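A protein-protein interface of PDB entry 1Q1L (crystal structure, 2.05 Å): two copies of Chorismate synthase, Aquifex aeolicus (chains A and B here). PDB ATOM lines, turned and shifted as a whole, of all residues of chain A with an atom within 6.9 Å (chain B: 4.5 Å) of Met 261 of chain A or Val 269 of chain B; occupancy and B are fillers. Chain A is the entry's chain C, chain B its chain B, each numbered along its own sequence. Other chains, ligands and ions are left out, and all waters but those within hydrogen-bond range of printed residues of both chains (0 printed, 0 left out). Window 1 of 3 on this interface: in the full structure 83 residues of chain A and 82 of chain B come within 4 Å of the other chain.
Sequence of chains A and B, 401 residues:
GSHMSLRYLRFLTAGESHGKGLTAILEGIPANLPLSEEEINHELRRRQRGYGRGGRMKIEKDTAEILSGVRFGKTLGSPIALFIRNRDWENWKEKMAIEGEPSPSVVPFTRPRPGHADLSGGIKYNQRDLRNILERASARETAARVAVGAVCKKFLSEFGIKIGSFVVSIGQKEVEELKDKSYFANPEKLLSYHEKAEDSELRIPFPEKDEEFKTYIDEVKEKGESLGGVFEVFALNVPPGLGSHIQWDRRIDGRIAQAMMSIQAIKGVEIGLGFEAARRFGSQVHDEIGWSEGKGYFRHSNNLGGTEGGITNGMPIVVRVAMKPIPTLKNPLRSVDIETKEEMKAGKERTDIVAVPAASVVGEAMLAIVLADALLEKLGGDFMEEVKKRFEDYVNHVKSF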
ATOM      1  N   ARG A 145     -14.818  16.734 -10.669  1.00  0.00           N
ATOM      2  CA  ARG A 145     -13.793  17.362  -9.849  1.00  0.00           C
ATOM      3  C   ARG A 145     -12.750  16.316  -9.492  1.00  0.00           C
ATOM      4  O   ARG A 145     -11.563  16.616  -9.401  1.00  0.00           O
ATOM      5  CB  ARG A 145     -14.422  17.966  -8.591  1.00  0.00           C
ATOM      6  CG  ARG A 145     -15.284  19.166  -8.912  1.00  0.00           C
ATOM      7  CD  ARG A 145     -16.252  19.532  -7.799  1.00  0.00           C
ATOM      8  NE  ARG A 145     -15.609  20.138  -6.647  1.00  0.00           N
ATOM      9  CZ  ARG A 145     -16.258  20.846  -5.730  1.00  0.00           C
ATOM     10  NH1 ARG A 145     -17.565  21.030  -5.843  1.00  0.00           N
ATOM     11  NH2 ARG A 145     -15.601  21.366  -4.700  1.00  0.00           N
ATOM     12  N   ILE A 256      -7.169  26.500   0.570  1.00  0.00           N
ATOM     13  CA  ILE A 256      -7.572  25.141   0.901  1.00  0.00           C
ATOM     14  C   ILE A 256      -8.987  25.167   1.474  1.00  0.00           C
ATOM     15  O   ILE A 256      -9.808  24.304   1.162  1.00  0.00           O
ATOM     16  CB  ILE A 256      -6.609  24.510   1.935  1.00  0.00           C
ATOM     17  CG1 ILE A 256      -5.280  24.170   1.257  1.00  0.00           C
ATOM     18  CG2 ILE A 256      -7.251  23.287   2.577  1.00  0.00           C
ATOM     19  CD1 ILE A 256      -4.260  23.507   2.181  1.00  0.00           C
ATOM     20  N   ALA A 257      -9.273  26.174   2.297  1.00  0.00           N
ATOM     21  CA  ALA A 257     -10.592  26.306   2.917  1.00  0.00           C
ATOM     22  C   ALA A 257     -11.726  26.444   1.896  1.00  0.00           C
ATOM     23  O   ALA A 257     -12.785  25.825   2.044  1.00  0.00           O
ATOM     24  CB  ALA A 257     -10.607  27.499   3.868  1.00  0.00           C
ATOM     25  N   GLN A 258     -11.516  27.259   0.865  1.00  0.00           N
ATOM     26  CA  GLN A 258     -12.551  27.426  -0.151  1.00  0.00           C
ATOM     27  C   GLN A 258     -12.761  26.119  -0.888  1.00  0.00           C
ATOM     28  O   GLN A 258     -13.891  25.696  -1.099  1.00  0.00           O
ATOM     29  CB  GLN A 258     -12.173  28.499  -1.180  1.00  0.00           C
ATOM     30  CG  GLN A 258     -13.322  28.800  -2.157  1.00  0.00           C
ATOM     31  CD  GLN A 258     -12.935  29.749  -3.279  1.00  0.00           C
ATOM     32  OE1 GLN A 258     -13.796  30.378  -3.900  1.00  0.00           O
ATOM     33  NE2 GLN A 258     -11.642  29.841  -3.560  1.00  0.00           N
ATOM     34  N   ALA A 259     -11.660  25.489  -1.286  1.00  0.00           N
ATOM     35  CA  ALA A 259     -11.716  24.229  -2.020  1.00  0.00           C
ATOM     36  C   ALA A 259     -12.502  23.159  -1.272  1.00  0.00           C
ATOM     37  O   ALA A 259     -13.364  22.504  -1.855  1.00  0.00           O
ATOM     38  CB  ALA A 259     -10.305  23.729  -2.312  1.00  0.00           C
ATOM     39  N   MET A 260     -12.194  22.976   0.011  1.00  0.00           N
ATOM     40  CA  MET A 260     -12.891  21.987   0.830  1.00  0.00           C
ATOM     41  C   MET A 260     -14.350  22.363   1.067  1.00  0.00           C
ATOM     42  O   MET A 260     -15.249  21.549   0.854  1.00  0.00           O
ATOM     43  CB  MET A 260     -12.196  21.815   2.192  1.00  0.00           C
ATOM     44  CG  MET A 260     -10.840  21.147   2.142  1.00  0.00           C
ATOM     45  SD  MET A 260     -10.840  19.479   1.159  1.00  0.00           S
ATOM     46  CE  MET A 260     -12.453  18.702   1.842  1.00  0.00           C
ATOM     47  N   MET A 261     -14.588  23.594   1.503  1.00  0.00           N
ATOM     48  CA  MET A 261     -15.953  24.035   1.773  1.00  0.00           C
ATOM     49  C   MET A 261     -16.834  24.098   0.522  1.00  0.00           C
ATOM     50  O   MET A 261     -18.061  24.168   0.633  1.00  0.00           O
ATOM     51  CB  MET A 261     -15.947  25.407   2.453  1.00  0.00           C
ATOM     52  CG  MET A 261     -17.277  25.788   3.096  1.00  0.00           C
ATOM     53  SD  MET A 261     -17.554  24.977   4.863  1.00  0.00           S
ATOM     54  CE  MET A 261     -16.452  26.205   5.879  1.00  0.00           C
ATOM     55  N   SER A 262     -16.226  24.079  -0.661  1.00  0.00           N
ATOM     56  CA  SER A 262     -17.005  24.133  -1.894  1.00  0.00           C
ATOM     57  C   SER A 262     -17.635  22.777  -2.188  1.00  0.00           C
ATOM     58  O   SER A 262     -18.513  22.664  -3.042  1.00  0.00           O
ATOM     59  CB  SER A 262     -16.130  24.545  -3.085  1.00  0.00           C
ATOM     60  OG  SER A 262     -15.215  23.521  -3.439  1.00  0.00           O
ATOM     61  N   ILE A 263     -17.175  21.745  -1.490  1.00  0.00           N
ATOM     62  CA  ILE A 263     -17.721  20.414  -1.697  1.00  0.00           C
ATOM     63  C   ILE A 263     -19.131  20.347  -1.117  1.00  0.00           C
ATOM     64  O   ILE A 263     -19.401  20.869  -0.035  1.00  0.00           O
ATOM     65  CB  ILE A 263     -16.822  19.340  -1.045  1.00  0.00           C
ATOM     66  CG1 ILE A 263     -15.410  19.434  -1.638  1.00  0.00           C
ATOM     67  CG2 ILE A 263     -17.410  17.946  -1.294  1.00  0.00           C
ATOM     68  CD1 ILE A 263     -14.384  18.521  -0.992  1.00  0.00           C
ATOM     69  N   GLN A 264     -20.033  19.715  -1.855  1.00  0.00           N
ATOM     70  CA  GLN A 264     -21.416  19.583  -1.431  1.00  0.00           C
ATOM     71  C   GLN A 264     -21.532  18.986  -0.030  1.00  0.00           C
ATOM     72  O   GLN A 264     -20.868  17.995   0.287  1.00  0.00           O
ATOM     73  CB  GLN A 264     -22.196  18.714  -2.431  1.00  0.00           C
ATOM     74  CG  GLN A 264     -22.527  19.410  -3.756  1.00  0.00           C
ATOM     75  CD  GLN A 264     -21.438  19.261  -4.807  1.00  0.00           C
ATOM     76  OE1 GLN A 264     -20.251  19.455  -4.531  1.00  0.00           O
ATOM     77  NE2 GLN A 264     -21.843  18.923  -6.028  1.00  0.00           N
ATOM     78  N   ALA A 265     -22.356  19.618   0.804  1.00  0.00           N
ATOM     79  CA  ALA A 265     -22.614  19.155   2.163  1.00  0.00           C
ATOM     80  C   ALA A 265     -21.526  19.438   3.200  1.00  0.00           C
ATOM     81  O   ALA A 265     -21.655  19.042   4.367  1.00  0.00           O
ATOM     82  CB  ALA A 265     -22.940  17.668   2.140  1.00  0.00           C
ATOM     83  N   ILE A 266     -20.456  20.114   2.801  1.00  0.00           N
ATOM     84  CA  ILE A 266     -19.415  20.425   3.768  1.00  0.00           C
ATOM     85  C   ILE A 266     -19.810  21.718   4.472  1.00  0.00           C
ATOM     86  O   ILE A 266     -20.125  22.718   3.824  1.00  0.00           O
ATOM     87  CB  ILE A 266     -18.028  20.570   3.090  1.00  0.00           C
ATOM     88  CG1 ILE A 266     -17.629  19.238   2.438  1.00  0.00           C
ATOM     89  CG2 ILE A 266     -16.969  21.009   4.112  1.00  0.00           C
ATOM     90  CD1 ILE A 266     -17.714  18.017   3.357  1.00  0.00           C
ATOM     91  N   LYS A 267     -19.826  21.687   5.803  1.00  0.00           N
ATOM     92  CA  LYS A 267     -20.211  22.862   6.578  1.00  0.00           C
ATOM     93  C   LYS A 267     -19.092  23.281   7.506  1.00  0.00           C
ATOM     94  O   LYS A 267     -19.188  24.301   8.196  1.00  0.00           O
ATOM     95  CB  LYS A 267     -21.458  22.566   7.422  1.00  0.00           C
ATOM     96  CG  LYS A 267     -22.667  22.080   6.626  1.00  0.00           C
ATOM     97  CD  LYS A 267     -23.116  23.083   5.560  1.00  0.00           C
ATOM     98  CE  LYS A 267     -23.644  24.382   6.156  1.00  0.00           C
ATOM     99  NZ  LYS A 267     -24.157  25.295   5.080  1.00  0.00           N
ATOM    100  N   GLY A 268     -18.030  22.489   7.530  1.00  0.00           N
ATOM    101  CA  GLY A 268     -16.929  22.816   8.404  1.00  0.00           C
ATOM    102  C   GLY A 268     -15.569  22.383   7.909  1.00  0.00           C
ATOM    103  O   GLY A 268     -15.393  21.315   7.309  1.00  0.00           O
ATOM    104  N   VAL A 269     -14.587  23.228   8.180  1.00  0.00           N
ATOM    105  CA  VAL A 269     -13.156  22.952   7.758  1.00  0.00           C
ATOM    106  C   VAL A 269     -12.074  23.576   8.806  1.00  0.00           C
ATOM    107  O   VAL A 269     -12.242  24.762   9.338  1.00  0.00           O
ATOM    108  CB  VAL A 269     -12.826  23.607   6.091  1.00  0.00           C
ATOM    109  CG1 VAL A 269     -11.072  23.144   5.553  1.00  0.00           C
ATOM    110  CG2 VAL A 269     -14.120  22.958   4.886  1.00  0.00           C
ATOM    111  N   GLU A 270     -11.026  22.814   9.072  1.00  0.00           N
ATOM    112  CA  GLU A 270      -9.987  23.278   9.960  1.00  0.00           C
ATOM    113  C   GLU A 270      -8.661  22.760   9.443  1.00  0.00           C
ATOM    114  O   GLU A 270      -8.590  21.695   8.825  1.00  0.00           O
ATOM    115  CB  GLU A 270     -10.257  22.820  11.396  1.00  0.00           C
ATOM    116  CG  GLU A 270     -10.486  21.342  11.578  1.00  0.00           C
ATOM    117  CD  GLU A 270     -11.196  21.029  12.895  1.00  0.00           C
ATOM    118  OE1 GLU A 270     -11.242  21.910  13.778  1.00  0.00           O
ATOM    119  OE2 GLU A 270     -11.704  19.902  13.052  1.00  0.00           O
ATOM    120  N   ILE A 271      -7.620  23.554   9.645  1.00  0.00           N
ATOM    121  CA  ILE A 271      -6.284  23.169   9.232  1.00  0.00           C
ATOM    122  C   ILE A 271      -5.585  22.837  10.537  1.00  0.00           C
ATOM    123  O   ILE A 271      -5.473  23.696  11.416  1.00  0.00           O
ATOM    124  CB  ILE A 271      -5.539  24.337   8.564  1.00  0.00           C
ATOM    125  CG1 ILE A 271      -6.383  24.901   7.416  1.00  0.00           C
ATOM    126  CG2 ILE A 271      -4.189  23.873   8.051  1.00  0.00           C
ATOM    127  CD1 ILE A 271      -6.815  23.876   6.393  1.00  0.00           C
ATOM    128  N   GLY A 274      -7.459  22.894  14.441  1.00  0.00           N
ATOM    129  CA  GLY A 274      -8.693  23.626  14.209  1.00  0.00           C
ATOM    130  C   GLY A 274      -9.300  24.268  15.444  1.00  0.00           C
ATOM    131  O   GLY A 274      -8.640  25.032  16.146  1.00  0.00           O
ATOM    132  N   PHE A 275     -10.568  23.960  15.700  1.00  0.00           N
ATOM    133  CA  PHE A 275     -11.273  24.511  16.848  1.00  0.00           C
ATOM    134  C   PHE A 275     -10.647  24.099  18.184  1.00  0.00           C
ATOM    135  O   PHE A 275     -10.712  24.851  19.157  1.00  0.00           O
ATOM    136  CB  PHE A 275     -12.759  24.124  16.783  1.00  0.00           C
ATOM    137  CG  PHE A 275     -13.565  24.989  15.836  1.00  0.00           C
ATOM    138  CD1 PHE A 275     -14.209  26.134  16.294  1.00  0.00           C
ATOM    139  CD2 PHE A 275     -13.621  24.695  14.472  1.00  0.00           C
ATOM    140  CE1 PHE A 275     -14.891  26.977  15.416  1.00  0.00           C
ATOM    141  CE2 PHE A 275     -14.302  25.535  13.582  1.00  0.00           C
ATOM    142  CZ  PHE A 275     -14.937  26.678  14.057  1.00  0.00           C
ATOM    143  N   VAL A 321     -12.362  17.888   7.684  1.00  0.00           N
ATOM    144  CA  VAL A 321     -13.583  18.315   7.020  1.00  0.00           C
ATOM    145  C   VAL A 321     -14.864  17.704   7.587  1.00  0.00           C
ATOM    146  O   VAL A 321     -14.962  16.487   7.758  1.00  0.00           O
ATOM    147  CB  VAL A 321     -13.498  17.989   5.519  1.00  0.00           C
ATOM    148  CG1 VAL A 321     -14.624  18.668   4.762  1.00  0.00           C
ATOM    149  CG2 VAL A 321     -12.148  18.419   4.985  1.00  0.00           C
ATOM    150  N   ALA A 322     -15.847  18.561   7.851  1.00  0.00           N
ATOM    151  CA  ALA A 322     -17.133  18.136   8.397  1.00  0.00           C
ATOM    152  C   ALA A 322     -18.251  18.155   7.354  1.00  0.00           C
ATOM    153  O   ALA A 322     -18.508  19.183   6.722  1.00  0.00           O
ATOM    154  CB  ALA A 322     -17.515  19.032   9.570  1.00  0.00           C
ATOM    155  N   ASP B 253     -20.470  29.517   0.467  1.00  0.00           N
ATOM    156  CA  ASP B 253     -19.793  28.948   1.627  1.00  0.00           C
ATOM    157  C   ASP B 253     -18.283  28.909   1.428  1.00  0.00           C
ATOM    158  O   ASP B 253     -17.519  29.271   2.325  1.00  0.00           O
ATOM    159  CB  ASP B 253     -20.340  27.549   1.913  1.00  0.00           C
ATOM    160  CG  ASP B 253     -20.725  26.805   0.652  1.00  0.00           C
ATOM    161  OD1 ASP B 253     -19.824  26.320  -0.069  1.00  0.00           O
ATOM    162  OD2 ASP B 253     -21.939  26.716   0.370  1.00  0.00           O
ATOM    163  N   GLY B 254     -17.857  28.482   0.245  1.00  0.00           N
ATOM    164  CA  GLY B 254     -16.439  28.431  -0.043  1.00  0.00           C
ATOM    165  C   GLY B 254     -15.832  29.820  -0.006  1.00  0.00           C
ATOM    166  O   GLY B 254     -14.734  30.007   0.518  1.00  0.00           O
ATOM    167  N   ALA B 257     -15.497  30.898   3.519  1.00  0.00           N
ATOM    168  CA  ALA B 257     -14.407  30.133   4.130  1.00  0.00           C
ATOM    169  C   ALA B 257     -13.018  30.703   3.830  1.00  0.00           C
ATOM    170  O   ALA B 257     -12.161  30.758   4.714  1.00  0.00           O
ATOM    171  CB  ALA B 257     -14.475  28.674   3.683  1.00  0.00           C
ATOM    172  N   MET B 260     -12.548  34.177   5.658  1.00  0.00           N
ATOM    173  CA  MET B 260     -12.327  33.999   7.095  1.00  0.00           C
ATOM    174  C   MET B 260     -10.985  33.352   7.411  1.00  0.00           C
ATOM    175  O   MET B 260     -10.183  33.903   8.167  1.00  0.00           O
ATOM    176  CB  MET B 260     -13.446  33.153   7.716  1.00  0.00           C
ATOM    177  CG  MET B 260     -14.805  33.844   7.840  1.00  0.00           C
ATOM    178  SD  MET B 260     -14.719  35.596   8.670  1.00  0.00           S
ATOM    179  CE  MET B 260     -13.584  35.177  10.166  1.00  0.00           C
ATOM    180  N   MET B 261     -10.746  32.183   6.827  1.00  0.00           N
ATOM    181  CA  MET B 261      -9.512  31.449   7.044  1.00  0.00           C
ATOM    182  C   MET B 261      -8.268  32.235   6.636  1.00  0.00           C
ATOM    183  O   MET B 261      -7.156  31.877   7.023  1.00  0.00           O
ATOM    184  CB  MET B 261      -9.553  30.128   6.276  1.00  0.00           C
ATOM    185  CG  MET B 261      -8.479  29.141   6.674  1.00  0.00           C
ATOM    186  SD  MET B 261      -8.885  28.257   8.362  1.00  0.00           S
ATOM    187  CE  MET B 261      -9.933  26.790   7.662  1.00  0.00           C
ATOM    188  N   ILE B 266      -6.343  32.270  12.205  1.00  0.00           N
ATOM    189  CA  ILE B 266      -7.573  31.494  12.054  1.00  0.00           C
ATOM    190  C   ILE B 266      -7.267  30.102  11.519  1.00  0.00           C
ATOM    191  O   ILE B 266      -6.698  29.956  10.444  1.00  0.00           O
ATOM    192  CB  ILE B 266      -8.574  32.195  11.103  1.00  0.00           C
ATOM    193  CG1 ILE B 266      -8.895  33.604  11.615  1.00  0.00           C
ATOM    194  CG2 ILE B 266      -9.834  31.351  10.967  1.00  0.00           C
ATOM    195  CD1 ILE B 266      -9.398  33.640  13.060  1.00  0.00           C
ATOM    196  N   GLY B 268      -9.782  27.525  11.821  1.00  0.00           N
ATOM    197  CA  GLY B 268     -11.011  26.789  11.653  1.00  0.00           C
ATOM    198  C   GLY B 268     -12.177  27.683  11.305  1.00  0.00           C
ATOM    199  O   GLY B 268     -12.296  28.811  11.790  1.00  0.00           O
ATOM    200  N   VAL B 269     -13.048  27.177  10.449  1.00  0.00           N
ATOM    201  CA  VAL B 269     -14.279  27.970  10.027  1.00  0.00           C
ATOM    202  C   VAL B 269     -15.541  26.969   9.798  1.00  0.00           C
ATOM    203  O   VAL B 269     -15.407  25.833   9.154  1.00  0.00           O
ATOM    204  CB  VAL B 269     -13.978  28.940   8.512  1.00  0.00           C
ATOM    205  CG1 VAL B 269     -12.551  30.135   8.786  1.00  0.00           C
ATOM    206  CG2 VAL B 269     -13.618  27.774   7.076  1.00  0.00           C
ATOM    207  N   GLU B 270     -16.689  27.379  10.313  1.00  0.00           N
ATOM    208  CA  GLU B 270     -17.901  26.601  10.179  1.00  0.00           C
ATOM    209  C   GLU B 270     -18.992  27.537   9.716  1.00  0.00           C
ATOM    210  O   GLU B 270     -19.007  28.719  10.059  1.00  0.00           O
ATOM    211  CB  GLU B 270     -18.312  26.009  11.522  1.00  0.00           C
ATOM    212  CG  GLU B 270     -17.516  24.805  11.970  1.00  0.00           C
ATOM    213  CD  GLU B 270     -17.899  24.388  13.373  1.00  0.00           C
ATOM    214  OE1 GLU B 270     -17.808  23.183  13.690  1.00  0.00           O
ATOM    215  OE2 GLU B 270     -18.287  25.286  14.153  1.00  0.00           O
ATOM    216  N   ILE B 271     -19.901  26.994   8.927  1.00  0.00           N
ATOM    217  CA  ILE B 271     -21.042  27.738   8.450  1.00  0.00           C
ATOM    218  C   ILE B 271     -22.169  27.066   9.219  1.00  0.00           C
ATOM    219  O   ILE B 271     -22.444  25.883   9.015  1.00  0.00           O
ATOM    220  CB  ILE B 271     -21.255  27.540   6.942  1.00  0.00           C
ATOM    221  CG1 ILE B 271     -20.048  28.082   6.174  1.00  0.00           C
ATOM    222  CG2 ILE B 271     -22.523  28.236   6.511  1.00  0.00           C
ATOM    223  CD1 ILE B 271     -19.748  29.542   6.460  1.00  0.00           C
ATOM    224  N   ARG B 320     -18.835  30.479  12.207  1.00  0.00           N
ATOM    225  CA  ARG B 320     -18.115  30.279  13.468  1.00  0.00           C
ATOM    226  C   ARG B 320     -16.645  30.209  13.073  1.00  0.00           C
ATOM    227  O   ARG B 320     -16.274  29.429  12.201  1.00  0.00           O
ATOM    228  CB  ARG B 320     -18.560  28.982  14.158  1.00  0.00           C
ATOM    229  CG  ARG B 320     -20.075  28.797  14.189  1.00  0.00           C
ATOM    230  CD  ARG B 320     -20.521  27.667  15.126  1.00  0.00           C
ATOM    231  NE  ARG B 320     -20.325  28.024  16.530  1.00  0.00           N
ATOM    232  CZ  ARG B 320     -19.297  27.627  17.274  1.00  0.00           C
ATOM    233  NH1 ARG B 320     -18.359  26.841  16.761  1.00  0.00           N
ATOM    234  NH2 ARG B 320     -19.196  28.037  18.534  1.00  0.00           N
ATOM    235  N   VAL B 321     -15.816  31.035  13.706  1.00  0.00           N
ATOM    236  CA  VAL B 321     -14.397  31.095  13.381  1.00  0.00           C
ATOM    237  C   VAL B 321     -13.487  30.806  14.579  1.00  0.00           C
ATOM    238  O   VAL B 321     -13.681  31.352  15.668  1.00  0.00           O
ATOM    239  CB  VAL B 321     -14.066  32.486  12.808  1.00  0.00           C
ATOM    240  CG1 VAL B 321     -12.659  32.512  12.248  1.00  0.00           C
ATOM    241  CG2 VAL B 321     -15.094  32.851  11.731  1.00  0.00           C
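The backbone carbonyl oxygen (O) of Val 269 of chain A is in hydrogen-bond range of the backbone NH (N) of Val 269 of chain B.
O of Lys 267 of chain A lies within hydrogen-bond range of N of Ile 271 of chain B.
The backbone carbonyl oxygen (O) of Met 261 of chain A lies close to the side-chain carboxylate (OD1) of Asp 253 of chain B, 2.9 Å away.
The side-chain sulfur (SD) of Met 261 of chain B is in hydrogen-bond range of the backbone NH (N) of Gly 268 of chain B (3.6 Å).
The guanidinium group of Arg 320 of chain B lies within salt-bridge range of the side-chain carboxylate of Glu 270 of chain B (3.0 Å).
O of Gln 258 of chain A sits close to OG of Ser 262 of chain A.
The backbone carbonyl oxygen (O) of Ala 322 of chain A sits at hydrogen-bond distance from the backbone NH (N) of Lys 267 of chain A.
O of Gly 268 of chain A lies within hydrogen-bond range of N of Ala 322 of chain A, 2.8 Å away.
The side-chain carboxylate of Glu 270 of chain A is in hydrogen-bond range of the backbone NH of Phe 275 of chain A (2.9 Å).
O of Ala 257 of chain A touches CB of Ala 257 of chain B (3.7 Å).
CA of Gly 254 of chain B touches CB of Met 261 of chain A (3.95 Å).
CB of Ala 257 of chain B touches CB of Met 261 of chain A (3.8 Å).
Met 261 of chain A touches Val 269 of chain B.
Lys 267 of chain A touches Glu 270 of chain B.
O of Val 269 of chain B touches CA of Gly 268 of chain A, 3.5 Å away.
Gly 268 of chain B touches Val 269 of chain A (CA to O, 3.3 Å).
C of Gly 268 of chain B touches CE2 of Phe 275 of chain A, at 3.8 Å.
Val 269 of chain B touches Phe 275 of chain A (N to CE2, 3.8 Å).
Arg 320 of chain B touches Phe 275 of chain A (O to CZ, 3.6 Å).
Of the printed residues of chain B, Met 261 of chain A touches Asp 253 (2.9 Å), Gly 254 (3.95 Å), Ala 257 (3.8 Å) and Val 269 (3.5 Å).
Of the printed residues of chain A, Val 269 of chain B touches Met 261, Gly 268, Val 269 and Phe 275.
Printed residues of chain A within 4 Å of Asp 253 of chain B: Met 261 (2.9 Å).
Of the printed residues of chain A, Gly 268 of chain B touches Val 269 (3.3 Å) and Phe 275 (3.8 Å).
Of the printed residues of chain B, Val 269 of chain A touches Met 261 (3.5 Å), Gly 268 (3.3 Å) and Val 269 (2.8 Å).
Ile 263 of chain A touches none of the printed residues of chain B.
Glu 270 of chain A touches none of the printed residues of chain B.
The nearest printed residue of chain A that does not touch Val 269 of chain B is Lys 267 of chain A (4.2 Å).
Of the 12 printed residues of chain B, 9 touch a printed residue of chain A.
Hydrophobic or aromatic side chains of chain B within 4 Å of the printed part of chain A: Ala 257, Met 261, Val 269 and Ile 271.
Along chain B the printed residues that touch a printed residue of chain A span positions 253 to 320.
Of the 21 printed residues of chain A, 7 touch a printed residue of chain B.
Among the printed residues, no Asp or Glu carboxylate lies within 4 Å of a Lys or Arg side-chain nitrogen of the other chain.
Ala 257 of chain A touches its own counterpart, Ala 257 of chain B.
Met 261 of chain A touches Val 269 of chain B, and with the chains exchanged Val 269 of chain A touches Met 261 of chain B.
Gly 268 of chain A touches Val 269 of chain B, and with the chains exchanged Val 269 of chain A touches Gly 268 of chain B.
Val 269 of chain B touches its own counterpart, Val 269 of chain A.
Of the 17 pairs that touch across the chains among the printed residues, 8 have their exchanged pair printed and touching as well.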
